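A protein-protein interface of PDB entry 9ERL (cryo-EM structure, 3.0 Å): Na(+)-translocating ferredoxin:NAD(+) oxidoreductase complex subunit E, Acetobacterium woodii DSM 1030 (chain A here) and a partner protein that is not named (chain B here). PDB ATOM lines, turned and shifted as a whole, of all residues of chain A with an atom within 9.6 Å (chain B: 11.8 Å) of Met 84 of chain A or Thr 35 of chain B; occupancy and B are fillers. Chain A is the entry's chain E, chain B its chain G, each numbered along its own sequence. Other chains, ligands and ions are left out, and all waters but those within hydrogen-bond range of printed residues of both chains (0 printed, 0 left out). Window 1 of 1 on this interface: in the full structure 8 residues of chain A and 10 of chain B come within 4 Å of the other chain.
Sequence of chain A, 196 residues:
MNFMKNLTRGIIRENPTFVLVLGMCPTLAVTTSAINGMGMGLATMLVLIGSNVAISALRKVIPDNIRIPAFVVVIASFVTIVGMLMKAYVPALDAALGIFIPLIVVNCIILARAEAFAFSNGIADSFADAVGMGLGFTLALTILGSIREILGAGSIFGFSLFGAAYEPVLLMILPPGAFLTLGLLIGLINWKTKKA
SD of Met 84 of chain A sits close to O of Thr 35 of chain B (3.3 Å).
Of the 20 printed residues of chain A, 5 touch a printed residue of chain B. Hydrophobic or aromatic side chains of chain A within 4 Å of the printed part of chain B: Ile 81, Met 84 and Ala 88. Of the 21 printed residues of chain B, 7 touch a printed residue of chain A. Hydrophobic or aromatic side chains of chain B within 4 Å of the printed part of chain A: Ala 28, Leu 32, Ile 43 and Met 46. Among the printed residues, no Asp or Glu carboxylate lies within 4 Å of a Lys or Arg side-chain nitrogen of the other chain.
The side-chain hydroxyl (OG1) of Thr 35 of chain B lies within hydrogen-bond range of the backbone carbonyl oxygen (O) of Ala 31 of chain B, at 3.2 Å.
Met 84 of chain A touches just these residues of chain B: Thr 35, Asn 36 and Thr 39. Printed residues of chain A within 4 Å of Thr 35 of chain B: Met 84. No residue of chain B comes within 4 Å of Thr 80 of chain A. No residue of chain B comes within 4 Å of Gly 83 of chain A. Lys 87 of chain A touches just one residue of chain B: Ile 43. Ala 88 of chain A touches three residues of chain B. Of the printed residues of chain A, Ile 43 of chain B touches Lys 87 and Ala 88. Printed residues of chain A within 4 Å of Asn 36 of chain B: Met 84. Printed residues of chain B within 4 Å of Ser 77 of chain A: Ala 28. Of the printed residues of chain A, Thr 39 of chain B touches Met 84 (3.4 Å) and Ala 88 (3.6 Å). Printed residues of chain B within 4 Å of Ile 81 of chain A: Leu 32 (3.9 Å). Val 90 of chain A touches none of the printed residues of chain B. Phe 78 of chain A touches none of the printed residues of chain B. The nearest printed residue of chain A that does not touch Thr 35 of chain B is Ile 81 of chain A (4.002 Å). The nearest printed residue of chain B that does not touch Ser 77 of chain A is Leu 32 of chain B (4.03 Å).
Among the printed residues, pairs that only touch across the chains: Ala 88 of chain A with Met 46 of chain B, Met 84 of chain A with Thr 39 of chain B, Ala 88 of chain A with Thr 39 of chain B, Lys 87 of chain A with Ile 43 of chain B, Ser 77 of chain A with Ala 28 of chain B, Ala 88 of chain A with Ile 43 of chain B, Met 84 of chain A with Asn 36 of chain B and Ile 81 of chain A with Leu 32 of chain B.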
ATOM      1  N   ALA A  76      15.926  17.983   5.151  1.00  0.00           N
ATOM      2  CA  ALA A  76      14.560  17.520   4.951  1.00  0.00           C
ATOM      3  C   ALA A  76      13.598  18.683   4.752  1.00  0.00           C
ATOM      4  O   ALA A  76      12.642  18.570   3.979  1.00  0.00           O
ATOM      5  CB  ALA A  76      14.124  16.656   6.131  1.00  0.00           C
ATOM      6  N   SER A  77      13.830  19.808   5.435  1.00  0.00           N
ATOM      7  CA  SER A  77      12.995  20.987   5.208  1.00  0.00           C
ATOM      8  C   SER A  77      13.126  21.480   3.771  1.00  0.00           C
ATOM      9  O   SER A  77      12.121  21.764   3.099  1.00  0.00           O
ATOM     10  CB  SER A  77      13.372  22.095   6.190  1.00  0.00           C
ATOM     11  OG  SER A  77      13.697  21.559   7.459  1.00  0.00           O
ATOM     12  N   PHE A  78      14.365  21.566   3.273  1.00  0.00           N
ATOM     13  CA  PHE A  78      14.561  22.023   1.898  1.00  0.00           C
ATOM     14  C   PHE A  78      13.961  21.042   0.894  1.00  0.00           C
ATOM     15  O   PHE A  78      13.341  21.454  -0.099  1.00  0.00           O
ATOM     16  CB  PHE A  78      16.048  22.243   1.626  1.00  0.00           C
ATOM     17  CG  PHE A  78      16.544  23.587   2.071  1.00  0.00           C
ATOM     18  CD1 PHE A  78      16.173  24.735   1.394  1.00  0.00           C
ATOM     19  CD2 PHE A  78      17.371  23.704   3.174  1.00  0.00           C
ATOM     20  CE1 PHE A  78      16.622  25.973   1.806  1.00  0.00           C
ATOM     21  CE2 PHE A  78      17.823  24.939   3.591  1.00  0.00           C
ATOM     22  CZ  PHE A  78      17.448  26.075   2.905  1.00  0.00           C
ATOM     23  N   VAL A  79      14.119  19.739   1.149  1.00  0.00           N
ATOM     24  CA  VAL A  79      13.560  18.717   0.267  1.00  0.00           C
ATOM     25  C   VAL A  79      12.039  18.807   0.238  1.00  0.00           C
ATOM     26  O   VAL A  79      11.421  18.705  -0.828  1.00  0.00           O
ATOM     27  CB  VAL A  79      14.045  17.320   0.701  1.00  0.00           C
ATOM     28  CG1 VAL A  79      13.142  16.228   0.149  1.00  0.00           C
ATOM     29  CG2 VAL A  79      15.477  17.097   0.256  1.00  0.00           C
ATOM     30  N   THR A  80      11.416  19.008   1.402  1.00  0.00           N
ATOM     31  CA  THR A  80       9.961  19.114   1.462  1.00  0.00           C
ATOM     32  C   THR A  80       9.458  20.333   0.701  1.00  0.00           C
ATOM     33  O   THR A  80       8.452  20.252  -0.014  1.00  0.00           O
ATOM     34  CB  THR A  80       9.497  19.167   2.918  1.00  0.00           C
ATOM     35  OG1 THR A  80      10.112  18.103   3.655  1.00  0.00           O
ATOM     36  CG2 THR A  80       7.989  19.029   3.003  1.00  0.00           C
ATOM     37  N   ILE A  81      10.147  21.471   0.832  1.00  0.00           N
ATOM     38  CA  ILE A  81       9.722  22.677   0.117  1.00  0.00           C
ATOM     39  C   ILE A  81       9.832  22.474  -1.393  1.00  0.00           C
ATOM     40  O   ILE A  81       8.907  22.799  -2.156  1.00  0.00           O
ATOM     41  CB  ILE A  81      10.534  23.894   0.591  1.00  0.00           C
ATOM     42  CG1 ILE A  81      10.104  24.296   2.003  1.00  0.00           C
ATOM     43  CG2 ILE A  81      10.370  25.060  -0.369  1.00  0.00           C
ATOM     44  CD1 ILE A  81      11.076  25.215   2.700  1.00  0.00           C
ATOM     45  N   VAL A  82      10.960  21.911  -1.845  1.00  0.00           N
ATOM     46  CA  VAL A  82      11.157  21.676  -3.275  1.00  0.00           C
ATOM     47  C   VAL A  82      10.121  20.690  -3.806  1.00  0.00           C
ATOM     48  O   VAL A  82       9.562  20.880  -4.895  1.00  0.00           O
ATOM     49  CB  VAL A  82      12.598  21.199  -3.540  1.00  0.00           C
ATOM     50  CG1 VAL A  82      12.727  20.583  -4.925  1.00  0.00           C
ATOM     51  CG2 VAL A  82      13.573  22.355  -3.383  1.00  0.00           C
ATOM     52  N   GLY A  83       9.838  19.633  -3.043  1.00  0.00           N
ATOM     53  CA  GLY A  83       8.853  18.656  -3.475  1.00  0.00           C
ATOM     54  C   GLY A  83       7.447  19.219  -3.538  1.00  0.00           C
ATOM     55  O   GLY A  83       6.679  18.881  -4.441  1.00  0.00           O
ATOM     56  N   MET A  84       7.088  20.084  -2.583  1.00  0.00           N
ATOM     57  CA  MET A  84       5.783  20.738  -2.629  1.00  0.00           C
ATOM     58  C   MET A  84       5.653  21.613  -3.869  1.00  0.00           C
ATOM     59  O   MET A  84       4.623  21.589  -4.556  1.00  0.00           O
ATOM     60  CB  MET A  84       5.568  21.570  -1.364  1.00  0.00           C
ATOM     61  CG  MET A  84       4.865  20.839  -0.236  1.00  0.00           C
ATOM     62  SD  MET A  84       4.753  21.852   1.251  1.00  0.00           S
ATOM     63  CE  MET A  84       4.111  20.668   2.426  1.00  0.00           C
ATOM     64  N   LEU A  85       6.698  22.389  -4.177  1.00  0.00           N
ATOM     65  CA  LEU A  85       6.655  23.236  -5.369  1.00  0.00           C
ATOM     66  C   LEU A  85       6.550  22.401  -6.642  1.00  0.00           C
ATOM     67  O   LEU A  85       5.775  22.732  -7.551  1.00  0.00           O
ATOM     68  CB  LEU A  85       7.889  24.136  -5.418  1.00  0.00           C
ATOM     69  CG  LEU A  85       7.912  25.316  -4.444  1.00  0.00           C
ATOM     70  CD1 LEU A  85       9.105  26.211  -4.723  1.00  0.00           C
ATOM     71  CD2 LEU A  85       6.616  26.107  -4.519  1.00  0.00           C
ATOM     72  N   MET A  86       7.318  21.310  -6.721  1.00  0.00           N
ATOM     73  CA  MET A  86       7.276  20.451  -7.903  1.00  0.00           C
ATOM     74  C   MET A  86       5.921  19.772  -8.052  1.00  0.00           C
ATOM     75  O   MET A  86       5.417  19.626  -9.171  1.00  0.00           O
ATOM     76  CB  MET A  86       8.395  19.412  -7.838  1.00  0.00           C
ATOM     77  CG  MET A  86       8.531  18.568  -9.094  1.00  0.00           C
ATOM     78  SD  MET A  86      10.093  17.673  -9.222  1.00  0.00           S
ATOM     79  CE  MET A  86      11.099  18.521  -8.006  1.00  0.00           C
ATOM     80  N   LYS A  87       5.316  19.344  -6.939  1.00  0.00           N
ATOM     81  CA  LYS A  87       3.979  18.764  -6.998  1.00  0.00           C
ATOM     82  C   LYS A  87       2.959  19.790  -7.469  1.00  0.00           C
ATOM     83  O   LYS A  87       2.035  19.459  -8.221  1.00  0.00           O
ATOM     84  CB  LYS A  87       3.577  18.218  -5.627  1.00  0.00           C
ATOM     85  CG  LYS A  87       4.219  16.894  -5.262  1.00  0.00           C
ATOM     86  CD  LYS A  87       3.453  16.176  -4.158  1.00  0.00           C
ATOM     87  CE  LYS A  87       3.164  17.093  -2.983  1.00  0.00           C
ATOM     88  NZ  LYS A  87       3.391  16.412  -1.680  1.00  0.00           N
ATOM     89  N   ALA A  88       3.106  21.042  -7.028  1.00  0.00           N
ATOM     90  CA  ALA A  88       2.165  22.080  -7.435  1.00  0.00           C
ATOM     91  C   ALA A  88       2.290  22.406  -8.918  1.00  0.00           C
ATOM     92  O   ALA A  88       1.278  22.619  -9.594  1.00  0.00           O
ATOM     93  CB  ALA A  88       2.375  23.339  -6.598  1.00  0.00           C
ATOM     94  N   TYR A  89       3.515  22.452  -9.447  1.00  0.00           N
ATOM     95  CA  TYR A  89       3.718  23.011 -10.779  1.00  0.00           C
ATOM     96  C   TYR A  89       4.143  22.006 -11.842  1.00  0.00           C
ATOM     97  O   TYR A  89       3.782  22.183 -13.006  1.00  0.00           O
ATOM     98  CB  TYR A  89       4.749  24.144 -10.719  1.00  0.00           C
ATOM     99  CG  TYR A  89       4.250  25.338  -9.941  1.00  0.00           C
ATOM    100  CD1 TYR A  89       3.187  26.100 -10.407  1.00  0.00           C
ATOM    101  CD2 TYR A  89       4.830  25.692  -8.730  1.00  0.00           C
ATOM    102  CE1 TYR A  89       2.721  27.188  -9.694  1.00  0.00           C
ATOM    103  CE2 TYR A  89       4.371  26.779  -8.010  1.00  0.00           C
ATOM    104  CZ  TYR A  89       3.317  27.523  -8.496  1.00  0.00           C
ATOM    105  OH  TYR A  89       2.858  28.605  -7.783  1.00  0.00           O
ATOM    106  N   VAL A  90       4.895  20.965 -11.492  1.00  0.00           N
ATOM    107  CA  VAL A  90       5.349  19.986 -12.482  1.00  0.00           C
ATOM    108  C   VAL A  90       4.883  18.594 -12.069  1.00  0.00           C
ATOM    109  O   VAL A  90       5.638  17.856 -11.420  1.00  0.00           O
ATOM    110  CB  VAL A  90       6.877  20.020 -12.655  1.00  0.00           C
ATOM    111  CG1 VAL A  90       7.286  19.243 -13.895  1.00  0.00           C
ATOM    112  CG2 VAL A  90       7.388  21.450 -12.735  1.00  0.00           C
ATOM    113  N   PRO A  91       3.662  18.187 -12.426  1.00  0.00           N
ATOM    114  CA  PRO A  91       3.172  16.878 -11.966  1.00  0.00           C
ATOM    115  C   PRO A  91       3.756  15.698 -12.727  1.00  0.00           C
ATOM    116  O   PRO A  91       3.842  14.600 -12.162  1.00  0.00           O
ATOM    117  CB  PRO A  91       1.656  16.987 -12.170  1.00  0.00           C
ATOM    118  CG  PRO A  91       1.508  17.954 -13.294  1.00  0.00           C
ATOM    119  CD  PRO A  91       2.626  18.949 -13.143  1.00  0.00           C
ATOM    120  N   ASP A  94       7.027  14.695 -11.211  1.00  0.00           N
ATOM    121  CA  ASP A  94       6.730  14.096  -9.915  1.00  0.00           C
ATOM    122  C   ASP A  94       6.273  12.652 -10.080  1.00  0.00           C
ATOM    123  O   ASP A  94       6.723  11.764  -9.347  1.00  0.00           O
ATOM    124  CB  ASP A  94       5.657  14.917  -9.200  1.00  0.00           C
ATOM    125  CG  ASP A  94       5.195  14.286  -7.895  1.00  0.00           C
ATOM    126  OD1 ASP A  94       4.093  14.643  -7.436  1.00  0.00           O
ATOM    127  OD2 ASP A  94       5.948  13.497  -7.285  1.00  0.00           O
ATOM    128  N   ILE A 101      11.854  11.343  -4.887  1.00  0.00           N
ATOM    129  CA  ILE A 101      11.784  12.768  -4.557  1.00  0.00           C
ATOM    130  C   ILE A 101      11.728  12.960  -3.040  1.00  0.00           C
ATOM    131  O   ILE A 101      12.414  13.856  -2.528  1.00  0.00           O
ATOM    132  CB  ILE A 101      10.613  13.455  -5.284  1.00  0.00           C
ATOM    133  CG1 ILE A 101      10.907  13.555  -6.782  1.00  0.00           C
ATOM    134  CG2 ILE A 101      10.339  14.837  -4.704  1.00  0.00           C
ATOM    135  CD1 ILE A 101       9.926  14.411  -7.546  1.00  0.00           C
ATOM    136  N   PRO A 102      10.959  12.176  -2.267  1.00  0.00           N
ATOM    137  CA  PRO A 102      11.159  12.216  -0.808  1.00  0.00           C
ATOM    138  C   PRO A 102      12.521  11.713  -0.359  1.00  0.00           C
ATOM    139  O   PRO A 102      12.933  12.017   0.767  1.00  0.00           O
ATOM    140  CB  PRO A 102      10.033  11.323  -0.270  1.00  0.00           C
ATOM    141  CG  PRO A 102       8.994  11.372  -1.300  1.00  0.00           C
ATOM    142  CD  PRO A 102       9.723  11.442  -2.603  1.00  0.00           C
ATOM    143  N   ILE A 104      15.524  12.419  -1.629  1.00  0.00           N
ATOM    144  CA  ILE A 104      16.660  13.308  -1.856  1.00  0.00           C
ATOM    145  C   ILE A 104      17.329  13.695  -0.542  1.00  0.00           C
ATOM    146  O   ILE A 104      18.504  14.077  -0.535  1.00  0.00           O
ATOM    147  CB  ILE A 104      16.219  14.560  -2.643  1.00  0.00           C
ATOM    148  CG1 ILE A 104      15.320  14.169  -3.813  1.00  0.00           C
ATOM    149  CG2 ILE A 104      17.417  15.321  -3.187  1.00  0.00           C
ATOM    150  CD1 ILE A 104      14.854  15.345  -4.639  1.00  0.00           C
ATOM    151  N   ALA B  26      11.485  24.274  15.567  1.00  0.00           N
ATOM    152  CA  ALA B  26      10.410  25.251  15.448  1.00  0.00           C
ATOM    153  C   ALA B  26      10.503  25.981  14.120  1.00  0.00           C
ATOM    154  O   ALA B  26       9.518  26.056  13.373  1.00  0.00           O
ATOM    155  CB  ALA B  26      10.462  26.235  16.616  1.00  0.00           C
ATOM    156  N   VAL B  27      11.717  26.418  13.762  1.00  0.00           N
ATOM    157  CA  VAL B  27      11.902  27.161  12.520  1.00  0.00           C
ATOM    158  C   VAL B  27      11.458  26.316  11.340  1.00  0.00           C
ATOM    159  O   VAL B  27      10.728  26.794  10.459  1.00  0.00           O
ATOM    160  CB  VAL B  27      13.364  27.621  12.378  1.00  0.00           C
ATOM    161  CG1 VAL B  27      13.563  28.346  11.056  1.00  0.00           C
ATOM    162  CG2 VAL B  27      13.750  28.517  13.540  1.00  0.00           C
ATOM    163  N   ALA B  28      11.814  25.024  11.352  1.00  0.00           N
ATOM    164  CA  ALA B  28      11.419  24.141  10.263  1.00  0.00           C
ATOM    165  C   ALA B  28       9.905  24.113  10.126  1.00  0.00           C
ATOM    166  O   ALA B  28       9.365  24.358   9.039  1.00  0.00           O
ATOM    167  CB  ALA B  28      11.974  22.737  10.494  1.00  0.00           C
ATOM    168  N   ALA B  29       9.204  23.919  11.248  1.00  0.00           N
ATOM    169  CA  ALA B  29       7.748  23.910  11.195  1.00  0.00           C
ATOM    170  C   ALA B  29       7.227  25.260  10.736  1.00  0.00           C
ATOM    171  O   ALA B  29       6.331  25.331   9.884  1.00  0.00           O
ATOM    172  CB  ALA B  29       7.171  23.533  12.559  1.00  0.00           C
ATOM    173  N   CYS B  30       7.858  26.342  11.212  1.00  0.00           N
ATOM    174  CA  CYS B  30       7.402  27.685  10.873  1.00  0.00           C
ATOM    175  C   CYS B  30       7.511  27.933   9.376  1.00  0.00           C
ATOM    176  O   CYS B  30       6.810  28.790   8.826  1.00  0.00           O
ATOM    177  CB  CYS B  30       8.202  28.720  11.668  1.00  0.00           C
ATOM    178  SG  CYS B  30       7.971  30.449  11.181  1.00  0.00           S
ATOM    179  N   ALA B  31       8.364  27.170   8.688  1.00  0.00           N
ATOM    180  CA  ALA B  31       8.347  27.230   7.234  1.00  0.00           C
ATOM    181  C   ALA B  31       7.249  26.339   6.667  1.00  0.00           C
ATOM    182  O   ALA B  31       6.357  26.820   5.953  1.00  0.00           O
ATOM    183  CB  ALA B  31       9.711  26.830   6.673  1.00  0.00           C
ATOM    184  N   LEU B  32       7.260  25.054   7.046  1.00  0.00           N
ATOM    185  CA  LEU B  32       6.548  24.037   6.277  1.00  0.00           C
ATOM    186  C   LEU B  32       5.050  24.287   6.251  1.00  0.00           C
ATOM    187  O   LEU B  32       4.427  24.188   5.186  1.00  0.00           O
ATOM    188  CB  LEU B  32       6.846  22.648   6.843  1.00  0.00           C
ATOM    189  CG  LEU B  32       8.267  22.112   6.644  1.00  0.00           C
ATOM    190  CD1 LEU B  32       8.287  20.599   6.750  1.00  0.00           C
ATOM    191  CD2 LEU B  32       8.842  22.557   5.309  1.00  0.00           C
ATOM    192  N   ALA B  33       4.473  24.659   7.398  1.00  0.00           N
ATOM    193  CA  ALA B  33       3.043  24.935   7.474  1.00  0.00           C
ATOM    194  C   ALA B  33       2.632  25.988   6.454  1.00  0.00           C
ATOM    195  O   ALA B  33       1.651  25.804   5.721  1.00  0.00           O
ATOM    196  CB  ALA B  33       2.670  25.376   8.889  1.00  0.00           C
ATOM    197  N   LEU B  34       3.402  27.079   6.354  1.00  0.00           N
ATOM    198  CA  LEU B  34       3.096  28.078   5.335  1.00  0.00           C
ATOM    199  C   LEU B  34       3.218  27.485   3.940  1.00  0.00           C
ATOM    200  O   LEU B  34       2.301  27.624   3.118  1.00  0.00           O
ATOM    201  CB  LEU B  34       4.005  29.296   5.489  1.00  0.00           C
ATOM    202  CG  LEU B  34       3.519  30.373   6.461  1.00  0.00           C
ATOM    203  CD1 LEU B  34       4.050  30.142   7.863  1.00  0.00           C
ATOM    204  CD2 LEU B  34       3.911  31.752   5.956  1.00  0.00           C
ATOM    205  N   THR B  35       4.305  26.753   3.681  1.00  0.00           N
ATOM    206  CA  THR B  35       4.455  26.104   2.384  1.00  0.00           C
ATOM    207  C   THR B  35       3.393  25.030   2.197  1.00  0.00           C
ATOM    208  O   THR B  35       3.085  24.637   1.065  1.00  0.00           O
ATOM    209  CB  THR B  35       5.859  25.513   2.251  1.00  0.00           C
ATOM    210  OG1 THR B  35       6.811  26.417   2.824  1.00  0.00           O
ATOM    211  CG2 THR B  35       6.214  25.295   0.786  1.00  0.00           C
ATOM    212  N   ASN B  36       2.806  24.557   3.300  1.00  0.00           N
ATOM    213  CA  ASN B  36       1.702  23.615   3.193  1.00  0.00           C
ATOM    214  C   ASN B  36       0.479  24.268   2.568  1.00  0.00           C
ATOM    215  O   ASN B  36      -0.220  23.643   1.766  1.00  0.00           O
ATOM    216  CB  ASN B  36       1.349  23.046   4.566  1.00  0.00           C
ATOM    217  CG  ASN B  36       0.164  22.100   4.512  1.00  0.00           C
ATOM    218  OD1 ASN B  36       0.049  21.280   3.602  1.00  0.00           O
ATOM    219  ND2 ASN B  36      -0.732  22.218   5.485  1.00  0.00           N
ATOM    220  N   TYR B  37       0.201  25.524   2.930  1.00  0.00           N
ATOM    221  CA  TYR B  37      -1.124  26.087   2.675  1.00  0.00           C
ATOM    222  C   TYR B  37      -1.424  26.222   1.186  1.00  0.00           C
ATOM    223  O   TYR B  37      -2.147  25.399   0.605  1.00  0.00           O
ATOM    224  CB  TYR B  37      -1.241  27.450   3.359  1.00  0.00           C
ATOM    225  CG  TYR B  37      -1.979  27.421   4.674  1.00  0.00           C
ATOM    226  CD1 TYR B  37      -1.806  26.375   5.569  1.00  0.00           C
ATOM    227  CD2 TYR B  37      -2.853  28.443   5.019  1.00  0.00           C
ATOM    228  CE1 TYR B  37      -2.484  26.349   6.774  1.00  0.00           C
ATOM    229  CE2 TYR B  37      -3.535  28.426   6.219  1.00  0.00           C
ATOM    230  CZ  TYR B  37      -3.347  27.377   7.094  1.00  0.00           C
ATOM    231  OH  TYR B  37      -4.024  27.358   8.291  1.00  0.00           O
ATOM    232  N   VAL B  38      -0.781  27.193   0.532  1.00  0.00           N
ATOM    233  CA  VAL B  38      -1.234  27.631  -0.787  1.00  0.00           C
ATOM    234  C   VAL B  38      -1.081  26.511  -1.806  1.00  0.00           C
ATOM    235  O   VAL B  38      -2.034  26.175  -2.526  1.00  0.00           O
ATOM    236  CB  VAL B  38      -0.500  28.920  -1.210  1.00  0.00           C
ATOM    237  CG1 VAL B  38      -0.946  30.076  -0.337  1.00  0.00           C
ATOM    238  CG2 VAL B  38       1.012  28.774  -1.091  1.00  0.00           C
ATOM    239  N   THR B  39       0.086  25.854  -1.800  1.00  0.00           N
ATOM    240  CA  THR B  39       0.348  24.732  -2.692  1.00  0.00           C
ATOM    241  C   THR B  39      -0.764  23.701  -2.612  1.00  0.00           C
ATOM    242  O   THR B  39      -1.314  23.299  -3.649  1.00  0.00           O
ATOM    243  CB  THR B  39       1.696  24.099  -2.341  1.00  0.00           C
ATOM    244  OG1 THR B  39       2.757  24.987  -2.716  1.00  0.00           O
ATOM    245  CG2 THR B  39       1.870  22.766  -3.042  1.00  0.00           C
ATOM    246  N   ALA B  40      -1.178  23.346  -1.385  1.00  0.00           N
ATOM    247  CA  ALA B  40      -2.194  22.313  -1.218  1.00  0.00           C
ATOM    248  C   ALA B  40      -3.448  22.663  -1.996  1.00  0.00           C
ATOM    249  O   ALA B  40      -3.915  21.860  -2.816  1.00  0.00           O
ATOM    250  CB  ALA B  40      -2.527  22.115   0.259  1.00  0.00           C
ATOM    251  N   GLY B  41      -3.930  23.901  -1.839  1.00  0.00           N
ATOM    252  CA  GLY B  41      -5.133  24.297  -2.548  1.00  0.00           C
ATOM    253  C   GLY B  41      -4.963  24.152  -4.042  1.00  0.00           C
ATOM    254  O   GLY B  41      -5.749  23.460  -4.703  1.00  0.00           O
ATOM    255  N   THR B  42      -3.850  24.682  -4.566  1.00  0.00           N
ATOM    256  CA  THR B  42      -3.584  24.579  -5.994  1.00  0.00           C
ATOM    257  C   THR B  42      -3.554  23.124  -6.418  1.00  0.00           C
ATOM    258  O   THR B  42      -4.233  22.741  -7.382  1.00  0.00           O
ATOM    259  CB  THR B  42      -2.265  25.269  -6.340  1.00  0.00           C
ATOM    260  OG1 THR B  42      -2.317  26.640  -5.927  1.00  0.00           O
ATOM    261  CG2 THR B  42      -2.008  25.205  -7.836  1.00  0.00           C
ATOM    262  N   ILE B  43      -2.869  22.285  -5.629  1.00  0.00           N
ATOM    263  CA  ILE B  43      -2.757  20.871  -5.960  1.00  0.00           C
ATOM    264  C   ILE B  43      -4.142  20.271  -6.104  1.00  0.00           C
ATOM    265  O   ILE B  43      -4.475  19.695  -7.152  1.00  0.00           O
ATOM    266  CB  ILE B  43      -1.926  20.135  -4.892  1.00  0.00           C
ATOM    267  CG1 ILE B  43      -0.433  20.386  -5.109  1.00  0.00           C
ATOM    268  CG2 ILE B  43      -2.222  18.641  -4.918  1.00  0.00           C
ATOM    269  CD1 ILE B  43       0.457  19.555  -4.216  1.00  0.00           C
ATOM    270  N   GLU B  44      -5.010  20.525  -5.114  1.00  0.00           N
ATOM    271  CA  GLU B  44      -6.350  19.958  -5.152  1.00  0.00           C
ATOM    272  C   GLU B  44      -7.073  20.400  -6.410  1.00  0.00           C
ATOM    273  O   GLU B  44      -7.568  19.559  -7.174  1.00  0.00           O
ATOM    274  CB  GLU B  44      -7.132  20.368  -3.905  1.00  0.00           C
ATOM    275  CG  GLU B  44      -8.144  19.338  -3.438  1.00  0.00           C
ATOM    276  CD  GLU B  44      -9.212  19.938  -2.546  1.00  0.00           C
ATOM    277  OE1 GLU B  44      -9.520  21.138  -2.709  1.00  0.00           O
ATOM    278  OE2 GLU B  44      -9.744  19.211  -1.681  1.00  0.00           O
ATOM    279  N   MET B  46      -5.863  21.412  -9.260  1.00  0.00           N
ATOM    280  CA  MET B  46      -5.294  20.786 -10.444  1.00  0.00           C
ATOM    281  C   MET B  46      -5.789  19.359 -10.572  1.00  0.00           C
ATOM    282  O   MET B  46      -6.290  18.965 -11.636  1.00  0.00           O
ATOM    283  CB  MET B  46      -3.768  20.833 -10.386  1.00  0.00           C
ATOM    284  CG  MET B  46      -3.078  20.066 -11.504  1.00  0.00           C
ATOM    285  SD  MET B  46      -1.444  20.710 -11.918  1.00  0.00           S
ATOM    286  CE  MET B  46      -1.568  22.402 -11.339  1.00  0.00           C
ATOM    287  N   ASN B  47      -5.779  18.617  -9.456  1.00  0.00           N
ATOM    288  CA  ASN B  47      -6.218  17.229  -9.493  1.00  0.00           C
ATOM    289  C   ASN B  47      -7.644  17.141 -10.003  1.00  0.00           C
ATOM    290  O   ASN B  47      -7.920  16.402 -10.960  1.00  0.00           O
ATOM    291  CB  ASN B  47      -6.101  16.596  -8.107  1.00  0.00           C
ATOM    292  CG  ASN B  47      -4.695  16.128  -7.797  1.00  0.00           C
ATOM    293  OD1 ASN B  47      -3.780  16.293  -8.606  1.00  0.00           O
ATOM    294  ND2 ASN B  47      -4.513  15.538  -6.621  1.00  0.00           N
